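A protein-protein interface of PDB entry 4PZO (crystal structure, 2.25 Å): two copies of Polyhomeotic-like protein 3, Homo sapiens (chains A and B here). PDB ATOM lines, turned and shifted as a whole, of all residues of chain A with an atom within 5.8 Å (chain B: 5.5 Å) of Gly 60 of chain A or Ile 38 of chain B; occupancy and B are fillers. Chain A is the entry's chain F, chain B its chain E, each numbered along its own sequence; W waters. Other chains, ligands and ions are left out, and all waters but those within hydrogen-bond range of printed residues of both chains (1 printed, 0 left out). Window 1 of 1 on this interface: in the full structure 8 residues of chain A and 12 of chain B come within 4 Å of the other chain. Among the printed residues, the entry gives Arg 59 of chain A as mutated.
Among the printed residues, merely in contact across the chains: Lys 58 of chain A with Gln 36 of chain B (3.4 Å), Arg 59 of chain A with Met 55 of chain B (3.6 Å), Gly 60 of chain A with Glu 37 of chain B (3.4 Å), Gly 60 of chain A with Ile 38 of chain B (3.97 Å), Gly 60 of chain A with Ala 42 of chain B (3.5 Å), Pro 61 of chain A with Gln 36 of chain B (3.5 Å), Pro 61 of chain A with Glu 37 of chain B (3.8 Å), Leu 63 of chain A with Ala 42 of chain B (3.5 Å) and Leu 63 of chain A with Leu 46 of chain B (3.6 Å).
OE2 of Glu 37 of chain B sits close to NZ of Lys 58 of chain A (2.4 Å). The side-chain carboxylate (OD2) of Asp 39 of chain B lies within salt-bridge range of the side-chain amino group (NZ) of Lys 64 of chain A (2.8 Å). NE2 of Gln 36 of chain B lies close to NH1 of Arg 59 of chain A. The backbone NH (N) of Gly 60 of chain A sits at hydrogen-bond distance from the backbone carbonyl oxygen (O) of Gln 36 of chain B, 2.9 Å away.
No position is printed for both chains.
Of the 15 printed residues of chain B, 7 touch a printed residue of chain A. Printed residues of chain B that touch a printed residue of chain A: Gln 36, Glu 37, Ile 38, Asp 39, Ala 42, Leu 46 and Met 55. Hydrophobic or aromatic side chains of chain B that line the printed part of chain A: Ile 38, Ala 42, Leu 46 and Met 55. Hydrophobic or aromatic side chains of chain A within 4 Å of the printed part of chain B: Pro 61 and Leu 63. Among the printed residues, 13 pairs touch across the chains. Among the printed residues, Asp or Glu carboxylates within 4 Å of a Lys or Arg side-chain nitrogen of the other chain: Lys 58 of chain A with Glu 37 of chain B (2.4 Å) and Lys 64 of chain A with Asp 39 of chain B (2.8 Å).
Printed residues of chain B within 4 Å of Gly 60 of chain A: Gln 36 (2.9 Å), Glu 37 (3.4 Å), Ile 38 (3.97 Å) and Ala 42 (3.5 Å). Ile 38 of chain B touches just one residue of chain A: Gly 60 (3.97 Å). Printed residues of chain B within 4 Å of Arg 59 of chain A: Gln 36 (3.1 Å) and Met 55 (3.6 Å). Of the printed residues of chain A, Glu 37 of chain B touches Lys 58 (2.4 Å), Gly 60 (3.4 Å) and Pro 61 (3.8 Å). Printed residues of chain A within 4 Å of Met 55 of chain B: Arg 59. Of the printed residues of chain A, Asp 39 of chain B touches Lys 64 (2.8 Å). Val 16 of chain B touches none of the printed residues of chain A. Ala 62 of chain A touches none of the printed residues of chain B. The nearest residue of chain A that does not touch Ile 38 of chain B is Arg 59 of chain A (4.9 Å). The nearest printed residue of chain B that does not touch Pro 61 of chain A is Ala 42 of chain B (5.2 Å).
Water W1 bridges the backbone carbonyl oxygen (O) of Glu 37 of chain B (2.5 Å) and the side-chain amino group (NZ) of Lys 64 of chain A (2.8 Å).
O of Phe 33 of chain B sits at hydrogen-bond distance from N of Ile 38 of chain B. OD1 of Asp 39 of chain B sits at hydrogen-bond distance from N of Ala 42 of chain B.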
ATOM      1  N   LYS A  58      15.209 -29.883 -26.182  1.00  0.00           N
ATOM      2  CA  LYS A  58      15.036 -29.170 -24.914  1.00  0.00           C
ATOM      3  C   LYS A  58      15.128 -30.129 -23.721  1.00  0.00           C
ATOM      4  O   LYS A  58      14.572 -31.225 -23.760  1.00  0.00           O
ATOM      5  CB  LYS A  58      13.699 -28.410 -24.909  1.00  0.00           C
ATOM      6  CG  LYS A  58      13.796 -26.989 -25.483  1.00  0.00           C
ATOM      7  CD  LYS A  58      12.448 -26.425 -25.923  1.00  0.00           C
ATOM      8  CE  LYS A  58      12.093 -26.876 -27.329  1.00  0.00           C
ATOM      9  NZ  LYS A  58      10.883 -26.184 -27.850  1.00  0.00           N
ATOM     10  N   ARG A  59      15.845 -29.725 -22.674  1.00  0.00           N
ATOM     11  CA  ARG A  59      16.130 -30.619 -21.547  1.00  0.00           C
ATOM     12  C   ARG A  59      14.885 -31.169 -20.861  1.00  0.00           C
ATOM     13  O   ARG A  59      14.885 -32.304 -20.379  1.00  0.00           O
ATOM     14  CB  ARG A  59      16.981 -29.903 -20.503  1.00  0.00           C
ATOM     15  CG  ARG A  59      18.257 -29.313 -21.043  1.00  0.00           C
ATOM     16  CD  ARG A  59      19.202 -30.367 -21.590  1.00  0.00           C
ATOM     17  NE  ARG A  59      20.460 -29.728 -21.961  1.00  0.00           N
ATOM     18  CZ  ARG A  59      20.716 -29.173 -23.143  1.00  0.00           C
ATOM     19  NH1 ARG A  59      19.814 -29.191 -24.114  1.00  0.00           N
ATOM     20  NH2 ARG A  59      21.895 -28.605 -23.350  1.00  0.00           N
ATOM     21  N   GLY A  60      13.839 -30.348 -20.808  1.00  0.00           N
ATOM     22  CA  GLY A  60      12.597 -30.707 -20.147  1.00  0.00           C
ATOM     23  C   GLY A  60      12.019 -32.012 -20.652  1.00  0.00           C
ATOM     24  O   GLY A  60      11.965 -32.994 -19.913  1.00  0.00           O
ATOM     25  N   PRO A  61      11.581 -32.030 -21.919  1.00  0.00           N
ATOM     26  CA  PRO A  61      11.106 -33.270 -22.539  1.00  0.00           C
ATOM     27  C   PRO A  61      12.198 -34.335 -22.628  1.00  0.00           C
ATOM     28  O   PRO A  61      11.888 -35.523 -22.583  1.00  0.00           O
ATOM     29  CB  PRO A  61      10.662 -32.819 -23.934  1.00  0.00           C
ATOM     30  CG  PRO A  61      11.340 -31.510 -24.161  1.00  0.00           C
ATOM     31  CD  PRO A  61      11.434 -30.873 -22.817  1.00  0.00           C
ATOM     32  N   ALA A  62      13.452 -33.911 -22.751  1.00  0.00           N
ATOM     33  CA  ALA A  62      14.575 -34.841 -22.811  1.00  0.00           C
ATOM     34  C   ALA A  62      14.697 -35.640 -21.514  1.00  0.00           C
ATOM     35  O   ALA A  62      14.998 -36.833 -21.534  1.00  0.00           O
ATOM     36  CB  ALA A  62      15.868 -34.095 -23.097  1.00  0.00           C
ATOM     37  N   LEU A  63      14.461 -34.971 -20.390  1.00  0.00           N
ATOM     38  CA  LEU A  63      14.490 -35.622 -19.084  1.00  0.00           C
ATOM     39  C   LEU A  63      13.358 -36.630 -18.938  1.00  0.00           C
ATOM     40  O   LEU A  63      13.548 -37.723 -18.405  1.00  0.00           O
ATOM     41  CB  LEU A  63      14.399 -34.582 -17.966  1.00  0.00           C
ATOM     42  CG  LEU A  63      15.664 -33.798 -17.620  1.00  0.00           C
ATOM     43  CD1 LEU A  63      15.290 -32.506 -16.924  1.00  0.00           C
ATOM     44  CD2 LEU A  63      16.576 -34.631 -16.739  1.00  0.00           C
ATOM     45  N   LYS A  64      12.177 -36.249 -19.414  1.00  0.00           N
ATOM     46  CA  LYS A  64      10.992 -37.083 -19.280  1.00  0.00           C
ATOM     47  C   LYS A  64      11.060 -38.305 -20.192  1.00  0.00           C
ATOM     48  O   LYS A  64      10.603 -39.388 -19.824  1.00  0.00           O
ATOM     49  CB  LYS A  64       9.734 -36.260 -19.570  1.00  0.00           C
ATOM     50  CG  LYS A  64       9.448 -35.202 -18.510  1.00  0.00           C
ATOM     51  CD  LYS A  64       8.231 -34.354 -18.854  1.00  0.00           C
ATOM     52  CE  LYS A  64       8.522 -33.394 -19.996  1.00  0.00           C
ATOM     53  NZ  LYS A  64       7.359 -32.509 -20.289  1.00  0.00           N
ATOM     54  N   ILE A  65      11.634 -38.132 -21.379  1.00  0.00           N
ATOM     55  CA  ILE A  65      11.834 -39.249 -22.294  1.00  0.00           C
ATOM     56  C   ILE A  65      12.832 -40.233 -21.695  1.00  0.00           C
ATOM     57  O   ILE A  65      12.654 -41.446 -21.784  1.00  0.00           O
ATOM     58  CB  ILE A  65      12.324 -38.773 -23.678  1.00  0.00           C
ATOM     59  CG1 ILE A  65      11.221 -37.984 -24.388  1.00  0.00           C
ATOM     60  CG2 ILE A  65      12.741 -39.955 -24.539  1.00  0.00           C
ATOM     61  CD1 ILE A  65      11.623 -37.448 -25.743  1.00  0.00           C
ATOM     62  N   THR B  12       3.252 -26.626 -14.082  1.00  0.00           N
ATOM     63  CA  THR B  12       3.437 -26.347 -15.501  1.00  0.00           C
ATOM     64  C   THR B  12       4.833 -25.792 -15.753  1.00  0.00           C
ATOM     65  O   THR B  12       5.637 -25.666 -14.830  1.00  0.00           O
ATOM     66  CB  THR B  12       2.393 -25.347 -16.023  1.00  0.00           C
ATOM     67  OG1 THR B  12       2.570 -24.083 -15.371  1.00  0.00           O
ATOM     68  CG2 THR B  12       0.987 -25.859 -15.754  1.00  0.00           C
ATOM     69  N   VAL B  13       5.119 -25.460 -17.006  1.00  0.00           N
ATOM     70  CA  VAL B  13       6.398 -24.856 -17.357  1.00  0.00           C
ATOM     71  C   VAL B  13       6.506 -23.467 -16.732  1.00  0.00           C
ATOM     72  O   VAL B  13       7.581 -23.052 -16.295  1.00  0.00           O
ATOM     73  CB  VAL B  13       6.576 -24.765 -18.886  1.00  0.00           C
ATOM     74  CG1 VAL B  13       7.916 -24.140 -19.233  1.00  0.00           C
ATOM     75  CG2 VAL B  13       6.458 -26.145 -19.512  1.00  0.00           C
ATOM     76  N   VAL B  16       7.063 -23.526 -12.839  1.00  0.00           N
ATOM     77  CA  VAL B  16       8.455 -23.778 -12.488  1.00  0.00           C
ATOM     78  C   VAL B  16       9.287 -22.505 -12.633  1.00  0.00           C
ATOM     79  O   VAL B  16      10.179 -22.241 -11.826  1.00  0.00           O
ATOM     80  CB  VAL B  16       9.051 -24.906 -13.356  1.00  0.00           C
ATOM     81  CG1 VAL B  16      10.549 -25.035 -13.136  1.00  0.00           C
ATOM     82  CG2 VAL B  16       8.357 -26.218 -13.045  1.00  0.00           C
ATOM     83  N   GLU B  32      15.661 -19.663 -18.469  1.00  0.00           N
ATOM     84  CA  GLU B  32      16.259 -20.793 -19.174  1.00  0.00           C
ATOM     85  C   GLU B  32      15.482 -22.075 -18.898  1.00  0.00           C
ATOM     86  O   GLU B  32      15.337 -22.926 -19.775  1.00  0.00           O
ATOM     87  CB  GLU B  32      17.727 -20.963 -18.775  1.00  0.00           C
ATOM     88  CG  GLU B  32      18.433 -22.141 -19.440  1.00  0.00           C
ATOM     89  CD  GLU B  32      18.684 -21.932 -20.925  1.00  0.00           C
ATOM     90  OE1 GLU B  32      18.389 -20.832 -21.441  1.00  0.00           O
ATOM     91  OE2 GLU B  32      19.184 -22.873 -21.581  1.00  0.00           O
ATOM     92  N   PHE B  33      14.981 -22.206 -17.674  1.00  0.00           N
ATOM     93  CA  PHE B  33      14.117 -23.322 -17.311  1.00  0.00           C
ATOM     94  C   PHE B  33      12.847 -23.309 -18.154  1.00  0.00           C
ATOM     95  O   PHE B  33      12.347 -24.355 -18.562  1.00  0.00           O
ATOM     96  CB  PHE B  33      13.760 -23.268 -15.826  1.00  0.00           C
ATOM     97  CG  PHE B  33      14.848 -23.763 -14.919  1.00  0.00           C
ATOM     98  CD1 PHE B  33      15.998 -23.017 -14.718  1.00  0.00           C
ATOM     99  CD2 PHE B  33      14.717 -24.972 -14.258  1.00  0.00           C
ATOM    100  CE1 PHE B  33      16.998 -23.473 -13.881  1.00  0.00           C
ATOM    101  CE2 PHE B  33      15.712 -25.431 -13.420  1.00  0.00           C
ATOM    102  CZ  PHE B  33      16.853 -24.682 -13.231  1.00  0.00           C
ATOM    103  N   ARG B  34      12.334 -22.111 -18.408  1.00  0.00           N
ATOM    104  CA  ARG B  34      11.136 -21.945 -19.220  1.00  0.00           C
ATOM    105  C   ARG B  34      11.448 -22.224 -20.687  1.00  0.00           C
ATOM    106  O   ARG B  34      10.611 -22.750 -21.422  1.00  0.00           O
ATOM    107  CB  ARG B  34      10.570 -20.535 -19.057  1.00  0.00           C
ATOM    108  CG  ARG B  34       9.054 -20.465 -19.081  1.00  0.00           C
ATOM    109  CD  ARG B  34       8.572 -19.023 -19.059  1.00  0.00           C
ATOM    110  NE  ARG B  34       8.652 -18.399 -20.376  1.00  0.00           N
ATOM    111  CZ  ARG B  34       7.632 -18.318 -21.226  1.00  0.00           C
ATOM    112  NH1 ARG B  34       6.450 -18.816 -20.891  1.00  0.00           N
ATOM    113  NH2 ARG B  34       7.793 -17.735 -22.406  1.00  0.00           N
ATOM    114  N   GLN B  36      13.801 -24.335 -21.896  1.00  0.00           N
ATOM    115  CA  GLN B  36      13.997 -25.767 -22.117  1.00  0.00           C
ATOM    116  C   GLN B  36      12.749 -26.579 -21.781  1.00  0.00           C
ATOM    117  O   GLN B  36      12.795 -27.809 -21.737  1.00  0.00           O
ATOM    118  CB  GLN B  36      15.191 -26.277 -21.305  1.00  0.00           C
ATOM    119  CG  GLN B  36      16.531 -25.674 -21.710  1.00  0.00           C
ATOM    120  CD  GLN B  36      16.914 -25.970 -23.149  1.00  0.00           C
ATOM    121  OE1 GLN B  36      16.384 -25.370 -24.085  1.00  0.00           O
ATOM    122  NE2 GLN B  36      17.845 -26.896 -23.331  1.00  0.00           N
ATOM    123  N   GLU B  37      11.643 -25.875 -21.550  1.00  0.00           N
ATOM    124  CA  GLU B  37      10.348 -26.489 -21.278  1.00  0.00           C
ATOM    125  C   GLU B  37      10.402 -27.457 -20.101  1.00  0.00           C
ATOM    126  O   GLU B  37       9.967 -28.604 -20.206  1.00  0.00           O
ATOM    127  CB  GLU B  37       9.827 -27.208 -22.525  1.00  0.00           C
ATOM    128  CG  GLU B  37       9.655 -26.303 -23.732  1.00  0.00           C
ATOM    129  CD  GLU B  37       9.141 -27.043 -24.953  1.00  0.00           C
ATOM    130  OE1 GLU B  37       8.543 -28.129 -24.788  1.00  0.00           O
ATOM    131  OE2 GLU B  37       9.345 -26.539 -26.078  1.00  0.00           O
ATOM    132  N   ILE B  38      10.937 -26.985 -18.981  1.00  0.00           N
ATOM    133  CA  ILE B  38      11.008 -27.795 -17.773  1.00  0.00           C
ATOM    134  C   ILE B  38       9.772 -27.591 -16.913  1.00  0.00           C
ATOM    135  O   ILE B  38       9.623 -26.556 -16.263  1.00  0.00           O
ATOM    136  CB  ILE B  38      12.252 -27.464 -16.938  1.00  0.00           C
ATOM    137  CG1 ILE B  38      13.523 -27.674 -17.757  1.00  0.00           C
ATOM    138  CG2 ILE B  38      12.287 -28.311 -15.671  1.00  0.00           C
ATOM    139  CD1 ILE B  38      14.751 -27.200 -17.038  1.00  0.00           C
ATOM    140  N   ASP B  39       8.880 -28.576 -16.922  1.00  0.00           N
ATOM    141  CA  ASP B  39       7.719 -28.552 -16.044  1.00  0.00           C
ATOM    142  C   ASP B  39       8.088 -29.156 -14.698  1.00  0.00           C
ATOM    143  O   ASP B  39       9.256 -29.451 -14.445  1.00  0.00           O
ATOM    144  CB  ASP B  39       6.539 -29.300 -16.669  1.00  0.00           C
ATOM    145  CG  ASP B  39       6.938 -30.636 -17.263  1.00  0.00           C
ATOM    146  OD1 ASP B  39       7.973 -31.198 -16.852  1.00  0.00           O
ATOM    147  OD2 ASP B  39       6.209 -31.128 -18.148  1.00  0.00           O
ATOM    148  N   GLY B  40       7.095 -29.331 -13.834  1.00  0.00           N
ATOM    149  CA  GLY B  40       7.334 -29.885 -12.516  1.00  0.00           C
ATOM    150  C   GLY B  40       7.841 -31.309 -12.597  1.00  0.00           C
ATOM    151  O   GLY B  40       8.594 -31.764 -11.735  1.00  0.00           O
ATOM    152  N   ALA B  42       9.798 -32.601 -15.075  1.00  0.00           N
ATOM    153  CA  ALA B  42      11.210 -32.542 -15.433  1.00  0.00           C
ATOM    154  C   ALA B  42      12.044 -31.964 -14.294  1.00  0.00           C
ATOM    155  O   ALA B  42      13.206 -32.326 -14.120  1.00  0.00           O
ATOM    156  CB  ALA B  42      11.404 -31.722 -16.699  1.00  0.00           C
ATOM    157  N   LEU B  43      11.439 -31.065 -13.523  1.00  0.00           N
ATOM    158  CA  LEU B  43      12.115 -30.421 -12.402  1.00  0.00           C
ATOM    159  C   LEU B  43      12.551 -31.434 -11.348  1.00  0.00           C
ATOM    160  O   LEU B  43      13.589 -31.271 -10.708  1.00  0.00           O
ATOM    161  CB  LEU B  43      11.202 -29.368 -11.768  1.00  0.00           C
ATOM    162  CG  LEU B  43      11.797 -28.500 -10.657  1.00  0.00           C
ATOM    163  CD1 LEU B  43      12.829 -27.538 -11.225  1.00  0.00           C
ATOM    164  CD2 LEU B  43      10.704 -27.747  -9.911  1.00  0.00           C
ATOM    165  N   LEU B  46      15.594 -33.719 -12.549  1.00  0.00           N
ATOM    166  CA  LEU B  46      16.900 -33.072 -12.585  1.00  0.00           C
ATOM    167  C   LEU B  46      17.833 -33.616 -11.512  1.00  0.00           C
ATOM    168  O   LEU B  46      17.409 -33.926 -10.399  1.00  0.00           O
ATOM    169  CB  LEU B  46      16.753 -31.559 -12.419  1.00  0.00           C
ATOM    170  CG  LEU B  46      16.379 -30.762 -13.668  1.00  0.00           C
ATOM    171  CD1 LEU B  46      16.021 -29.331 -13.304  1.00  0.00           C
ATOM    172  CD2 LEU B  46      17.522 -30.783 -14.666  1.00  0.00           C
ATOM    173  N   MET B  55      22.426 -27.421 -18.941  1.00  0.00           N
ATOM    174  CA  MET B  55      21.746 -26.162 -19.225  1.00  0.00           C
ATOM    175  C   MET B  55      22.678 -24.953 -19.262  1.00  0.00           C
ATOM    176  O   MET B  55      22.220 -23.824 -19.442  1.00  0.00           O
ATOM    177  CB  MET B  55      20.646 -25.922 -18.191  1.00  0.00           C
ATOM    178  CG  MET B  55      20.390 -27.099 -17.271  1.00  0.00           C
ATOM    179  SD  MET B  55      18.658 -27.165 -16.799  1.00  0.00           S
ATOM    180  CE  MET B  55      17.911 -26.886 -18.404  1.00  0.00           C
HETATM  181  O   HOH W   1       8.177 -29.995 -21.221  1.00  0.00           O
